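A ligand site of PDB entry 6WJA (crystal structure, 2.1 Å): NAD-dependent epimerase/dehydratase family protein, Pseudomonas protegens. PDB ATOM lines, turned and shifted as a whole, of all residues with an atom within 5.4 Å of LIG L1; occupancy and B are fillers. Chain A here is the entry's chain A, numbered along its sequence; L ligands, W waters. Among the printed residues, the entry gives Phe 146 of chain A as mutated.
Water W16 lies within hydrogen-bond range of O2 of LIG L1, O of Ala 81 and N of Val 83.
Water W14 bridges O13 of LIG L1 (2.7 Å) and O of Tyr 187 (2.8 Å).
Water W8 lies within hydrogen-bond range of the backbone carbonyl oxygen (O) of Ser 188, an oxygen (O13) of LIG L1 and the guanidinium group (NH1) of Arg 273.
Water W2 bridges the guanidinium group of Arg 273 (2.8 Å) and an oxygen (O13) of LIG L1 (2.9 Å).
Water W13 bridges N of Thr 205 (2.6 Å) and O8 of LIG L1 (3.1 Å).
Water W5 lies within hydrogen-bond range of the backbone NH (N) of Ile 277, the guanidinium group (NH2) of Arg 214, the side-chain carboxylate (OD1) of Asp 276 and an oxygen (O16) of LIG L1.
NH2 of Arg 214 is in salt-bridge range of OD1 of Asp 276 (3.0 Å).
The backbone carbonyl oxygen (O) of Ile 277 lies within hydrogen-bond range of the guanidinium group (NH1) of Arg 214 (2.8 Å).
OD2 of Asp 276 sits at hydrogen-bond distance from NE2 of Gln 212.
The side-chain amide nitrogen (NE2) of Gln 212 sits at hydrogen-bond distance from the backbone carbonyl oxygen (O) of Phe 207, at 2.8 Å.
The backbone carbonyl oxygen of Gln 212 lies within hydrogen-bond range of the backbone NH of Leu 250, at 3.0 Å.
NH2 of Arg 273 lies within hydrogen-bond range of O of Pro 186.
Val 83 touches LIG L1 (CG2 to O2, 3.2 Å).
CB of Ala 123 touches C6 of LIG L1, at 3.7 Å.
Tyr 187 touches LIG L1 (O to C8, 3.6 Å).
Ser 188 touches LIG L1.
Gly 189 touches LIG L1 (CA to O14, 3.4 Å).
CE1 of Phe 194 touches N3 of LIG L1 (3.6 Å).
Leu 206 touches LIG L1 (CA to O7, 3.6 Å).
Leu 250 touches LIG L1 (CD1 to O10, 3.4 Å).
Arg 273 touches LIG L1.
Ile 277 touches LIG L1 (CD1 to O5, 3.99 Å).
Within 4 Å of LIG L1: Val 83, Ala 123, Asn 175, Tyr 187, Ser 188, Gly 189, Val 190, Phe 194, Thr 205, Leu 206, Phe 207, Gln 212, Arg 214, Leu 250, Arg 273, Asp 276 and Ile 277.
The guanidinium group (NE) of Arg 214 is in salt-bridge range of an oxygen (O17) of LIG L1 (2.7 Å).
A nitrogen (N3) of LIG L1 sits at hydrogen-bond distance from the backbone carbonyl oxygen (O) of Thr 205, 2.8 Å away.
The side-chain carboxylate of Asp 276 lies within hydrogen-bond range of an oxygen (O11) of LIG L1 (2.8 Å).
N of Val 190 is in hydrogen-bond range of O14 of LIG L1, at 2.8 Å.
The backbone NH of Phe 207 sits at hydrogen-bond distance from an oxygen (O7) of LIG L1, 2.9 Å away.
The side-chain amide nitrogen (ND2) of Asn 175 is in hydrogen-bond range of an oxygen (O17) of LIG L1.
O11 of LIG L1 is in hydrogen-bond range of NE2 of Gln 212.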
ATOM      1  N   ALA A  81      29.083 -17.803 -19.443  1.00  0.00           N
ATOM      2  CA  ALA A  81      28.913 -16.698 -20.378  1.00  0.00           C
ATOM      3  C   ALA A  81      27.628 -15.938 -20.110  1.00  0.00           C
ATOM      4  O   ALA A  81      27.538 -14.746 -20.415  1.00  0.00           O
ATOM      5  CB  ALA A  81      28.927 -17.228 -21.821  1.00  0.00           C
ATOM      6  N   VAL A  83      25.123 -13.723 -18.567  1.00  0.00           N
ATOM      7  CA  VAL A  83      25.015 -12.682 -17.563  1.00  0.00           C
ATOM      8  C   VAL A  83      23.925 -13.016 -16.554  1.00  0.00           C
ATOM      9  O   VAL A  83      24.085 -12.832 -15.338  1.00  0.00           O
ATOM     10  CB  VAL A  83      24.764 -11.328 -18.253  1.00  0.00           C
ATOM     11  CG1 VAL A  83      24.343 -10.282 -17.238  1.00  0.00           C
ATOM     12  CG2 VAL A  83      26.024 -10.887 -18.992  1.00  0.00           C
ATOM     13  N   ALA A 122      32.233  -6.413 -23.601  1.00  0.00           N
ATOM     14  CA  ALA A 122      31.670  -5.078 -23.669  1.00  0.00           C
ATOM     15  C   ALA A 122      30.773  -4.752 -22.470  1.00  0.00           C
ATOM     16  O   ALA A 122      30.549  -3.570 -22.189  1.00  0.00           O
ATOM     17  CB  ALA A 122      30.877  -4.891 -24.971  1.00  0.00           C
ATOM     18  N   ALA A 123      30.300  -5.767 -21.743  1.00  0.00           N
ATOM     19  CA  ALA A 123      29.517  -5.525 -20.532  1.00  0.00           C
ATOM     20  C   ALA A 123      30.241  -4.667 -19.481  1.00  0.00           C
ATOM     21  O   ALA A 123      29.566  -4.087 -18.620  1.00  0.00           O
ATOM     22  CB  ALA A 123      29.112  -6.861 -19.874  1.00  0.00           C
ATOM     23  N   GLY A 126      28.772  -1.142 -19.063  1.00  0.00           N
ATOM     24  CA  GLY A 126      27.386  -0.868 -18.688  1.00  0.00           C
ATOM     25  C   GLY A 126      26.613  -0.212 -19.817  1.00  0.00           C
ATOM     26  O   GLY A 126      26.721  -0.593 -20.990  1.00  0.00           O
ATOM     27  N   PHE A 146      28.845 -10.883 -13.463  1.00  0.00           N
ATOM     28  CA  PHE A 146      29.630 -11.268 -14.628  1.00  0.00           C
ATOM     29  C   PHE A 146      30.511 -10.109 -15.114  1.00  0.00           C
ATOM     30  O   PHE A 146      31.705 -10.276 -15.328  1.00  0.00           O
ATOM     31  CB  PHE A 146      28.697 -11.735 -15.764  1.00  0.00           C
ATOM     32  CG  PHE A 146      29.402 -11.873 -17.107  1.00  0.00           C
ATOM     33  CD1 PHE A 146      29.470 -10.797 -17.993  1.00  0.00           C
ATOM     34  CD2 PHE A 146      30.017 -13.067 -17.448  1.00  0.00           C
ATOM     35  CE1 PHE A 146      30.137 -10.919 -19.217  1.00  0.00           C
ATOM     36  CE2 PHE A 146      30.691 -13.188 -18.665  1.00  0.00           C
ATOM     37  CZ  PHE A 146      30.753 -12.107 -19.545  1.00  0.00           C
ATOM     38  N   ASN A 175      29.526  -8.268 -30.049  1.00  0.00           N
ATOM     39  CA  ASN A 175      28.494  -9.307 -30.234  1.00  0.00           C
ATOM     40  C   ASN A 175      28.980 -10.372 -31.213  1.00  0.00           C
ATOM     41  O   ASN A 175      28.864 -10.209 -32.434  1.00  0.00           O
ATOM     42  CB  ASN A 175      27.186  -8.670 -30.675  1.00  0.00           C
ATOM     43  CG  ASN A 175      26.560  -7.817 -29.587  1.00  0.00           C
ATOM     44  OD1 ASN A 175      27.047  -6.719 -29.293  1.00  0.00           O
ATOM     45  ND2 ASN A 175      25.494  -8.324 -28.975  1.00  0.00           N
ATOM     46  N   GLN A 181      27.063 -21.517 -31.685  1.00  0.00           N
ATOM     47  CA  GLN A 181      26.580 -20.666 -30.611  1.00  0.00           C
ATOM     48  C   GLN A 181      25.217 -21.176 -30.156  1.00  0.00           C
ATOM     49  O   GLN A 181      24.259 -21.210 -30.942  1.00  0.00           O
ATOM     50  CB  GLN A 181      26.506 -19.204 -31.024  1.00  0.00           C
ATOM     51  CG  GLN A 181      26.057 -18.310 -29.862  1.00  0.00           C
ATOM     52  CD  GLN A 181      26.088 -16.818 -30.184  1.00  0.00           C
ATOM     53  OE1 GLN A 181      25.703 -16.404 -31.270  1.00  0.00           O
ATOM     54  NE2 GLN A 181      26.543 -16.014 -29.228  1.00  0.00           N
ATOM     55  N   PRO A 186      16.504 -17.989 -23.739  1.00  0.00           N
ATOM     56  CA  PRO A 186      15.918 -16.704 -24.160  1.00  0.00           C
ATOM     57  C   PRO A 186      16.930 -15.580 -24.219  1.00  0.00           C
ATOM     58  O   PRO A 186      16.718 -14.600 -24.942  1.00  0.00           O
ATOM     59  CB  PRO A 186      14.845 -16.435 -23.089  1.00  0.00           C
ATOM     60  CG  PRO A 186      14.540 -17.790 -22.513  1.00  0.00           C
ATOM     61  CD  PRO A 186      15.843 -18.528 -22.534  1.00  0.00           C
ATOM     62  N   TYR A 187      18.038 -15.695 -23.478  1.00  0.00           N
ATOM     63  CA  TYR A 187      19.085 -14.693 -23.471  1.00  0.00           C
ATOM     64  C   TYR A 187      20.270 -15.080 -24.340  1.00  0.00           C
ATOM     65  O   TYR A 187      21.304 -14.407 -24.293  1.00  0.00           O
ATOM     66  CB  TYR A 187      19.543 -14.440 -22.036  1.00  0.00           C
ATOM     67  CG  TYR A 187      18.451 -13.855 -21.173  1.00  0.00           C
ATOM     68  CD1 TYR A 187      18.126 -12.501 -21.238  1.00  0.00           C
ATOM     69  CD2 TYR A 187      17.723 -14.667 -20.304  1.00  0.00           C
ATOM     70  CE1 TYR A 187      17.113 -11.977 -20.459  1.00  0.00           C
ATOM     71  CE2 TYR A 187      16.717 -14.148 -19.531  1.00  0.00           C
ATOM     72  CZ  TYR A 187      16.410 -12.810 -19.613  1.00  0.00           C
ATOM     73  OH  TYR A 187      15.402 -12.293 -18.823  1.00  0.00           O
ATOM     74  N   SER A 188      20.147 -16.145 -25.140  1.00  0.00           N
ATOM     75  CA  SER A 188      21.158 -16.444 -26.130  1.00  0.00           C
ATOM     76  C   SER A 188      21.252 -15.307 -27.133  1.00  0.00           C
ATOM     77  O   SER A 188      20.369 -14.432 -27.207  1.00  0.00           O
ATOM     78  CB  SER A 188      20.840 -17.759 -26.846  1.00  0.00           C
ATOM     79  OG  SER A 188      20.758 -18.814 -25.907  1.00  0.00           O
ATOM     80  N   GLY A 189      22.351 -15.273 -27.888  1.00  0.00           N
ATOM     81  CA  GLY A 189      22.536 -14.213 -28.858  1.00  0.00           C
ATOM     82  C   GLY A 189      21.381 -14.108 -29.820  1.00  0.00           C
ATOM     83  O   GLY A 189      20.791 -15.134 -30.190  1.00  0.00           O
ATOM     84  N   VAL A 190      21.010 -12.886 -30.204  1.00  0.00           N
ATOM     85  CA  VAL A 190      19.816 -12.695 -31.025  1.00  0.00           C
ATOM     86  C   VAL A 190      19.979 -13.358 -32.387  1.00  0.00           C
ATOM     87  O   VAL A 190      19.005 -13.862 -32.968  1.00  0.00           O
ATOM     88  CB  VAL A 190      19.487 -11.195 -31.177  1.00  0.00           C
ATOM     89  CG1 VAL A 190      20.623 -10.451 -31.875  1.00  0.00           C
ATOM     90  CG2 VAL A 190      18.182 -11.000 -31.931  1.00  0.00           C
ATOM     91  N   ILE A 191      21.203 -13.399 -32.914  1.00  0.00           N
ATOM     92  CA  ILE A 191      21.406 -14.015 -34.222  1.00  0.00           C
ATOM     93  C   ILE A 191      21.195 -15.518 -34.129  1.00  0.00           C
ATOM     94  O   ILE A 191      20.544 -16.114 -35.004  1.00  0.00           O
ATOM     95  CB  ILE A 191      22.787 -13.644 -34.776  1.00  0.00           C
ATOM     96  CG1 ILE A 191      22.794 -12.180 -35.241  1.00  0.00           C
ATOM     97  CG2 ILE A 191      23.135 -14.553 -35.949  1.00  0.00           C
ATOM     98  CD1 ILE A 191      24.122 -11.726 -35.809  1.00  0.00           C
ATOM     99  N   ILE A 193      19.247 -17.059 -32.100  1.00  0.00           N
ATOM    100  CA  ILE A 193      17.824 -17.325 -31.886  1.00  0.00           C
ATOM    101  C   ILE A 193      17.042 -17.100 -33.176  1.00  0.00           C
ATOM    102  O   ILE A 193      16.260 -17.954 -33.605  1.00  0.00           O
ATOM    103  CB  ILE A 193      17.265 -16.478 -30.736  1.00  0.00           C
ATOM    104  CG1 ILE A 193      17.981 -16.808 -29.424  1.00  0.00           C
ATOM    105  CG2 ILE A 193      15.761 -16.695 -30.604  1.00  0.00           C
ATOM    106  CD1 ILE A 193      17.453 -16.031 -28.225  1.00  0.00           C
ATOM    107  N   PHE A 194      17.240 -15.933 -33.806  1.00  0.00           N
ATOM    108  CA  PHE A 194      16.508 -15.622 -35.029  1.00  0.00           C
ATOM    109  C   PHE A 194      16.848 -16.627 -36.140  1.00  0.00           C
ATOM    110  O   PHE A 194      15.966 -17.025 -36.911  1.00  0.00           O
ATOM    111  CB  PHE A 194      16.801 -14.194 -35.491  1.00  0.00           C
ATOM    112  CG  PHE A 194      16.129 -13.129 -34.653  1.00  0.00           C
ATOM    113  CD1 PHE A 194      15.350 -13.459 -33.543  1.00  0.00           C
ATOM    114  CD2 PHE A 194      16.244 -11.776 -34.999  1.00  0.00           C
ATOM    115  CE1 PHE A 194      14.730 -12.469 -32.789  1.00  0.00           C
ATOM    116  CE2 PHE A 194      15.616 -10.787 -34.252  1.00  0.00           C
ATOM    117  CZ  PHE A 194      14.868 -11.139 -33.140  1.00  0.00           C
ATOM    118  N   THR A 205      10.442 -13.460 -31.863  1.00  0.00           N
ATOM    119  CA  THR A 205       9.929 -12.377 -31.057  1.00  0.00           C
ATOM    120  C   THR A 205      10.938 -11.249 -31.087  1.00  0.00           C
ATOM    121  O   THR A 205      12.130 -11.471 -30.825  1.00  0.00           O
ATOM    122  CB  THR A 205       9.642 -12.808 -29.616  1.00  0.00           C
ATOM    123  OG1 THR A 205       8.628 -13.824 -29.625  1.00  0.00           O
ATOM    124  CG2 THR A 205       9.149 -11.612 -28.802  1.00  0.00           C
ATOM    125  N   LEU A 206      10.471 -10.059 -31.443  1.00  0.00           N
ATOM    126  CA  LEU A 206      11.296  -8.862 -31.426  1.00  0.00           C
ATOM    127  C   LEU A 206      10.938  -8.057 -30.186  1.00  0.00           C
ATOM    128  O   LEU A 206       9.764  -7.716 -29.987  1.00  0.00           O
ATOM    129  CB  LEU A 206      11.061  -8.050 -32.712  1.00  0.00           C
ATOM    130  CG  LEU A 206      11.804  -6.734 -32.897  1.00  0.00           C
ATOM    131  CD1 LEU A 206      13.309  -6.970 -33.014  1.00  0.00           C
ATOM    132  CD2 LEU A 206      11.251  -6.010 -34.125  1.00  0.00           C
ATOM    133  N   PHE A 207      11.919  -7.789 -29.341  1.00  0.00           N
ATOM    134  CA  PHE A 207      11.710  -7.013 -28.118  1.00  0.00           C
ATOM    135  C   PHE A 207      12.020  -5.552 -28.432  1.00  0.00           C
ATOM    136  O   PHE A 207      13.179  -5.140 -28.460  1.00  0.00           O
ATOM    137  CB  PHE A 207      12.590  -7.543 -26.985  1.00  0.00           C
ATOM    138  CG  PHE A 207      12.225  -8.948 -26.554  1.00  0.00           C
ATOM    139  CD1 PHE A 207      10.957  -9.219 -26.070  1.00  0.00           C
ATOM    140  CD2 PHE A 207      13.143  -9.973 -26.638  1.00  0.00           C
ATOM    141  CE1 PHE A 207      10.601 -10.517 -25.676  1.00  0.00           C
ATOM    142  CE2 PHE A 207      12.803 -11.266 -26.246  1.00  0.00           C
ATOM    143  CZ  PHE A 207      11.529 -11.539 -25.769  1.00  0.00           C
ATOM    144  N   GLN A 212      17.126  -1.066 -32.599  1.00  0.00           N
ATOM    145  CA  GLN A 212      18.385  -1.282 -31.895  1.00  0.00           C
ATOM    146  C   GLN A 212      19.486  -1.730 -32.856  1.00  0.00           C
ATOM    147  O   GLN A 212      19.246  -2.526 -33.773  1.00  0.00           O
ATOM    148  CB  GLN A 212      18.236  -2.353 -30.803  1.00  0.00           C
ATOM    149  CG  GLN A 212      17.089  -2.146 -29.864  1.00  0.00           C
ATOM    150  CD  GLN A 212      15.914  -3.035 -30.210  1.00  0.00           C
ATOM    151  OE1 GLN A 212      15.289  -2.870 -31.266  1.00  0.00           O
ATOM    152  NE2 GLN A 212      15.596  -3.979 -29.321  1.00  0.00           N
ATOM    153  N   ARG A 214      23.620  -3.221 -33.265  1.00  0.00           N
ATOM    154  CA  ARG A 214      24.690  -3.948 -32.619  1.00  0.00           C
ATOM    155  C   ARG A 214      25.874  -4.066 -33.564  1.00  0.00           C
ATOM    156  O   ARG A 214      25.724  -4.035 -34.790  1.00  0.00           O
ATOM    157  CB  ARG A 214      24.246  -5.360 -32.166  1.00  0.00           C
ATOM    158  CG  ARG A 214      23.223  -5.354 -31.041  1.00  0.00           C
ATOM    159  CD  ARG A 214      23.852  -4.811 -29.770  1.00  0.00           C
ATOM    160  NE  ARG A 214      22.991  -4.962 -28.601  1.00  0.00           N
ATOM    161  CZ  ARG A 214      22.048  -4.087 -28.247  1.00  0.00           C
ATOM    162  NH1 ARG A 214      21.846  -2.993 -28.995  1.00  0.00           N
ATOM    163  NH2 ARG A 214      21.299  -4.312 -27.166  1.00  0.00           N
ATOM    164  N   LEU A 250      18.235  -4.515 -35.764  1.00  0.00           N
ATOM    165  CA  LEU A 250      17.546  -5.798 -35.707  1.00  0.00           C
ATOM    166  C   LEU A 250      16.597  -5.959 -36.880  1.00  0.00           C
ATOM    167  O   LEU A 250      16.417  -7.080 -37.390  1.00  0.00           O
ATOM    168  CB  LEU A 250      16.793  -5.955 -34.376  1.00  0.00           C
ATOM    169  CG  LEU A 250      17.678  -5.963 -33.118  1.00  0.00           C
ATOM    170  CD1 LEU A 250      16.851  -6.277 -31.848  1.00  0.00           C
ATOM    171  CD2 LEU A 250      18.816  -6.936 -33.284  1.00  0.00           C
ATOM    172  N   ARG A 273      13.392  -4.859 -23.746  1.00  0.00           N
ATOM    173  CA  ARG A 273      13.985  -5.420 -22.537  1.00  0.00           C
ATOM    174  C   ARG A 273      14.444  -4.312 -21.610  1.00  0.00           C
ATOM    175  O   ARG A 273      15.004  -3.299 -22.041  1.00  0.00           O
ATOM    176  CB  ARG A 273      15.168  -6.318 -22.899  1.00  0.00           C
ATOM    177  CG  ARG A 273      14.761  -7.731 -23.288  1.00  0.00           C
ATOM    178  CD  ARG A 273      15.942  -8.692 -23.329  1.00  0.00           C
ATOM    179  NE  ARG A 273      15.488 -10.054 -23.607  1.00  0.00           N
ATOM    180  CZ  ARG A 273      16.223 -10.998 -24.184  1.00  0.00           C
ATOM    181  NH1 ARG A 273      17.469 -10.752 -24.545  1.00  0.00           N
ATOM    182  NH2 ARG A 273      15.696 -12.194 -24.398  1.00  0.00           N
ATOM    183  N   ASP A 276      18.033  -2.603 -21.724  1.00  0.00           N
ATOM    184  CA  ASP A 276      18.567  -2.847 -23.055  1.00  0.00           C
ATOM    185  C   ASP A 276      19.329  -1.621 -23.544  1.00  0.00           C
ATOM    186  O   ASP A 276      18.903  -0.481 -23.312  1.00  0.00           O
ATOM    187  CB  ASP A 276      17.417  -3.187 -24.006  1.00  0.00           C
ATOM    188  CG  ASP A 276      17.880  -3.747 -25.338  1.00  0.00           C
ATOM    189  OD1 ASP A 276      18.945  -4.398 -25.389  1.00  0.00           O
ATOM    190  OD2 ASP A 276      17.161  -3.529 -26.336  1.00  0.00           O
ATOM    191  N   ILE A 277      20.484  -1.836 -24.165  1.00  0.00           N
ATOM    192  CA  ILE A 277      21.156  -0.748 -24.858  1.00  0.00           C
ATOM    193  C   ILE A 277      20.558  -0.631 -26.246  1.00  0.00           C
ATOM    194  O   ILE A 277      20.439  -1.636 -26.972  1.00  0.00           O
ATOM    195  CB  ILE A 277      22.676  -0.986 -24.919  1.00  0.00           C
ATOM    196  CG1 ILE A 277      23.261  -1.131 -23.501  1.00  0.00           C
ATOM    197  CG2 ILE A 277      23.369   0.148 -25.667  1.00  0.00           C
ATOM    198  CD1 ILE A 277      24.746  -1.452 -23.474  1.00  0.00           C
HETATM  199  C1  LIG L   1      25.016  -8.702 -24.892  1.00  0.00           C
HETATM  200  C2  LIG L   1      25.190  -9.999 -24.147  1.00  0.00           C
HETATM  201  C3  LIG L   1      24.726  -9.784 -22.727  1.00  0.00           C
HETATM  202  C4  LIG L   1      25.537  -8.691 -22.060  1.00  0.00           C
HETATM  203  C5  LIG L   1      25.417  -7.412 -22.870  1.00  0.00           C
HETATM  204  C6  LIG L   1      26.444  -6.421 -22.362  1.00  0.00           C
HETATM  205  C7  LIG L   1      25.077 -12.021 -25.412  1.00  0.00           C
HETATM  206  C8  LIG L   1      24.232 -13.127 -26.014  1.00  0.00           C
HETATM  207  N1  LIG L   1      24.443 -11.054 -24.740  1.00  0.00           N
HETATM  208  O1  LIG L   1      23.641  -8.420 -24.938  1.00  0.00           O
HETATM  209  O2  LIG L   1      24.833 -10.999 -22.010  1.00  0.00           O
HETATM  210  O3  LIG L   1      26.890  -9.077 -21.979  1.00  0.00           O
HETATM  211  O4  LIG L   1      25.713  -7.649 -24.249  1.00  0.00           O
HETATM  212  O5  LIG L   1      26.184  -5.131 -22.880  1.00  0.00           O
HETATM  213  O6  LIG L   1      26.293 -11.995 -25.531  1.00  0.00           O
HETATM  214  N2  LIG L   1      16.410  -9.669 -28.824  1.00  0.00           N
HETATM  215  C9  LIG L   1      15.150  -9.799 -29.439  1.00  0.00           C
HETATM  216  N3  LIG L   1      14.515 -11.010 -29.529  1.00  0.00           N
HETATM  217  C10 LIG L   1      15.133 -12.077 -29.027  1.00  0.00           C
HETATM  218  C11 LIG L   1      16.498 -12.000 -28.368  1.00  0.00           C
HETATM  219  C12 LIG L   1      17.072 -10.740 -28.322  1.00  0.00           C
HETATM  220  O7  LIG L   1      14.594  -8.825 -29.891  1.00  0.00           O
HETATM  221  O8  LIG L   1      14.592 -13.157 -29.115  1.00  0.00           O
HETATM  222  C13 LIG L   1      17.014  -8.403 -28.766  1.00  0.00           C
HETATM  223  C14 LIG L   1      17.467  -8.027 -27.398  1.00  0.00           C
HETATM  224  O9  LIG L   1      16.406  -7.459 -26.591  1.00  0.00           O
HETATM  225  C15 LIG L   1      18.527  -6.970 -27.694  1.00  0.00           C
HETATM  226  C16 LIG L   1      19.130  -7.417 -29.025  1.00  0.00           C
HETATM  227  O10 LIG L   1      18.189  -8.384 -29.564  1.00  0.00           O
HETATM  228  O11 LIG L   1      17.875  -5.689 -27.936  1.00  0.00           O
HETATM  229  C17 LIG L   1      20.470  -8.014 -28.833  1.00  0.00           C
HETATM  230  O12 LIG L   1      20.372  -9.045 -27.880  1.00  0.00           O
HETATM  231  P1  LIG L   1      21.641  -9.879 -27.460  1.00  0.00           P
HETATM  232  O13 LIG L   1      21.350 -10.553 -26.153  1.00  0.00           O
HETATM  233  O14 LIG L   1      22.040 -10.874 -28.531  1.00  0.00           O
HETATM  234  O15 LIG L   1      22.861  -8.900 -27.254  1.00  0.00           O
HETATM  235  P2  LIG L   1      23.062  -7.725 -26.221  1.00  0.00           P
HETATM  236  O16 LIG L   1      21.758  -7.059 -25.921  1.00  0.00           O
HETATM  237  O17 LIG L   1      24.010  -6.682 -26.772  1.00  0.00           O
HETATM  238  P1  LG2 L   2      30.406 -20.722 -24.189  1.00  0.00           P
HETATM  239  O1  LG2 L   2      29.502 -20.957 -23.008  1.00  0.00           O
HETATM  240  O2  LG2 L   2      30.050 -21.575 -25.378  1.00  0.00           O
HETATM  241  O3  LG2 L   2      31.968 -20.959 -23.867  1.00  0.00           O
HETATM  242  C1  LG2 L   2      32.233 -20.922 -22.467  1.00  0.00           C
HETATM  243  C2  LG2 L   2      33.007 -22.201 -22.176  1.00  0.00           C
HETATM  244  O4  LG2 L   2      33.633 -22.192 -20.890  1.00  0.00           O
HETATM  245  C3  LG2 L   2      32.125 -23.456 -22.257  1.00  0.00           C
HETATM  246  O5  LG2 L   2      32.784 -24.434 -23.051  1.00  0.00           O
HETATM  247  C4  LG2 L   2      32.031 -23.905 -20.777  1.00  0.00           C
HETATM  248  O6  LG2 L   2      31.898 -25.320 -20.660  1.00  0.00           O
HETATM  249  C5  LG2 L   2      33.396 -23.430 -20.240  1.00  0.00           C
HETATM  250  N1  LG2 L   2      33.404 -23.202 -18.794  1.00  0.00           N
HETATM  251  C6  LG2 L   2      32.507 -22.477 -18.071  1.00  0.00           C
HETATM  252  N2  LG2 L   2      32.790 -22.446 -16.787  1.00  0.00           N
HETATM  253  C7  LG2 L   2      33.930 -23.178 -16.661  1.00  0.00           C
HETATM  254  C8  LG2 L   2      34.733 -23.540 -15.558  1.00  0.00           C
HETATM  255  N3  LG2 L   2      34.440 -23.117 -14.278  1.00  0.00           N
HETATM  256  N4  LG2 L   2      35.804 -24.285 -15.815  1.00  0.00           N
HETATM  257  C9  LG2 L   2      36.072 -24.675 -17.048  1.00  0.00           C
HETATM  258  N5  LG2 L   2      35.398 -24.427 -18.165  1.00  0.00           N
HETATM  259  C10 LG2 L   2      34.327 -23.660 -17.910  1.00  0.00           C
HETATM  260  O7  LG2 L   2      30.279 -19.192 -24.671  1.00  0.00           O
HETATM  261  P2  LG2 L   2      31.283 -18.349 -25.577  1.00  0.00           P
HETATM  262  O8  LG2 L   2      32.195 -19.227 -26.478  1.00  0.00           O
HETATM  263  O9  LG2 L   2      30.375 -17.401 -26.369  1.00  0.00           O
HETATM  264  O10 LG2 L   2      32.171 -17.518 -24.528  1.00  0.00           O
HETATM  265  C11 LG2 L   2      33.584 -17.705 -24.546  1.00  0.00           C
HETATM  266  C12 LG2 L   2      34.219 -16.502 -23.791  1.00  0.00           C
HETATM  267  O11 LG2 L   2      33.917 -15.262 -24.487  1.00  0.00           O
HETATM  268  C13 LG2 L   2      33.574 -16.349 -22.395  1.00  0.00           C
HETATM  269  O12 LG2 L   2      34.561 -15.915 -21.450  1.00  0.00           O
HETATM  270  C14 LG2 L   2      32.522 -15.243 -22.627  1.00  0.00           C
HETATM  271  O13 LG2 L   2      32.127 -14.581 -21.418  1.00  0.00           O
HETATM  272  C15 LG2 L   2      33.310 -14.349 -23.594  1.00  0.00           C
HETATM  273  N6  LG2 L   2      32.425 -13.462 -24.373  1.00  0.00           N
HETATM  274  C16 LG2 L   2      31.620 -13.939 -25.338  1.00  0.00           C
HETATM  275  C17 LG2 L   2      30.806 -13.076 -26.085  1.00  0.00           C
HETATM  276  C18 LG2 L   2      29.906 -13.541 -27.169  1.00  0.00           C
HETATM  277  O14 LG2 L   2      29.829 -14.733 -27.461  1.00  0.00           O
HETATM  278  N7  LG2 L   2      29.204 -12.625 -27.822  1.00  0.00           N
HETATM  279  C19 LG2 L   2      30.838 -11.698 -25.787  1.00  0.00           C
HETATM  280  C20 LG2 L   2      31.678 -11.254 -24.768  1.00  0.00           C
HETATM  281  C21 LG2 L   2      32.468 -12.167 -24.090  1.00  0.00           C
HETATM  282  O   HOH W   1      22.272 -11.372 -21.193  1.00  0.00           O
HETATM  283  O   HOH W   2      19.634  -8.938 -24.436  1.00  0.00           O
HETATM  284  O   HOH W   3      28.040 -11.587 -21.858  1.00  0.00           O
HETATM  285  O   HOH W   4      24.722 -11.067 -29.607  1.00  0.00           O
HETATM  286  O   HOH W   5      22.071  -4.170 -24.260  1.00  0.00           O
HETATM  287  O   HOH W   6      24.952  -4.674 -25.337  1.00  0.00           O
HETATM  288  O   HOH W   7      27.875 -10.249 -26.886  1.00  0.00           O
HETATM  289  O   HOH W   8      19.172 -12.302 -26.284  1.00  0.00           O
HETATM  290  O   HOH W   9      14.965  -4.978 -26.306  1.00  0.00           O
HETATM  291  O   HOH W  10      27.093  -3.280 -21.264  1.00  0.00           O
HETATM  292  O   HOH W  11      19.338  -6.513 -24.062  1.00  0.00           O
HETATM  293  O   HOH W  12      29.456  -8.263 -23.183  1.00  0.00           O
HETATM  294  O   HOH W  13      12.585 -14.625 -30.909  1.00  0.00           O
HETATM  295  O   HOH W  14      21.386 -11.672 -23.725  1.00  0.00           O
HETATM  296  O   HOH W  15      22.580  -8.057 -20.430  1.00  0.00           O
HETATM  297  O   HOH W  16      25.208 -13.448 -21.527  1.00  0.00           O
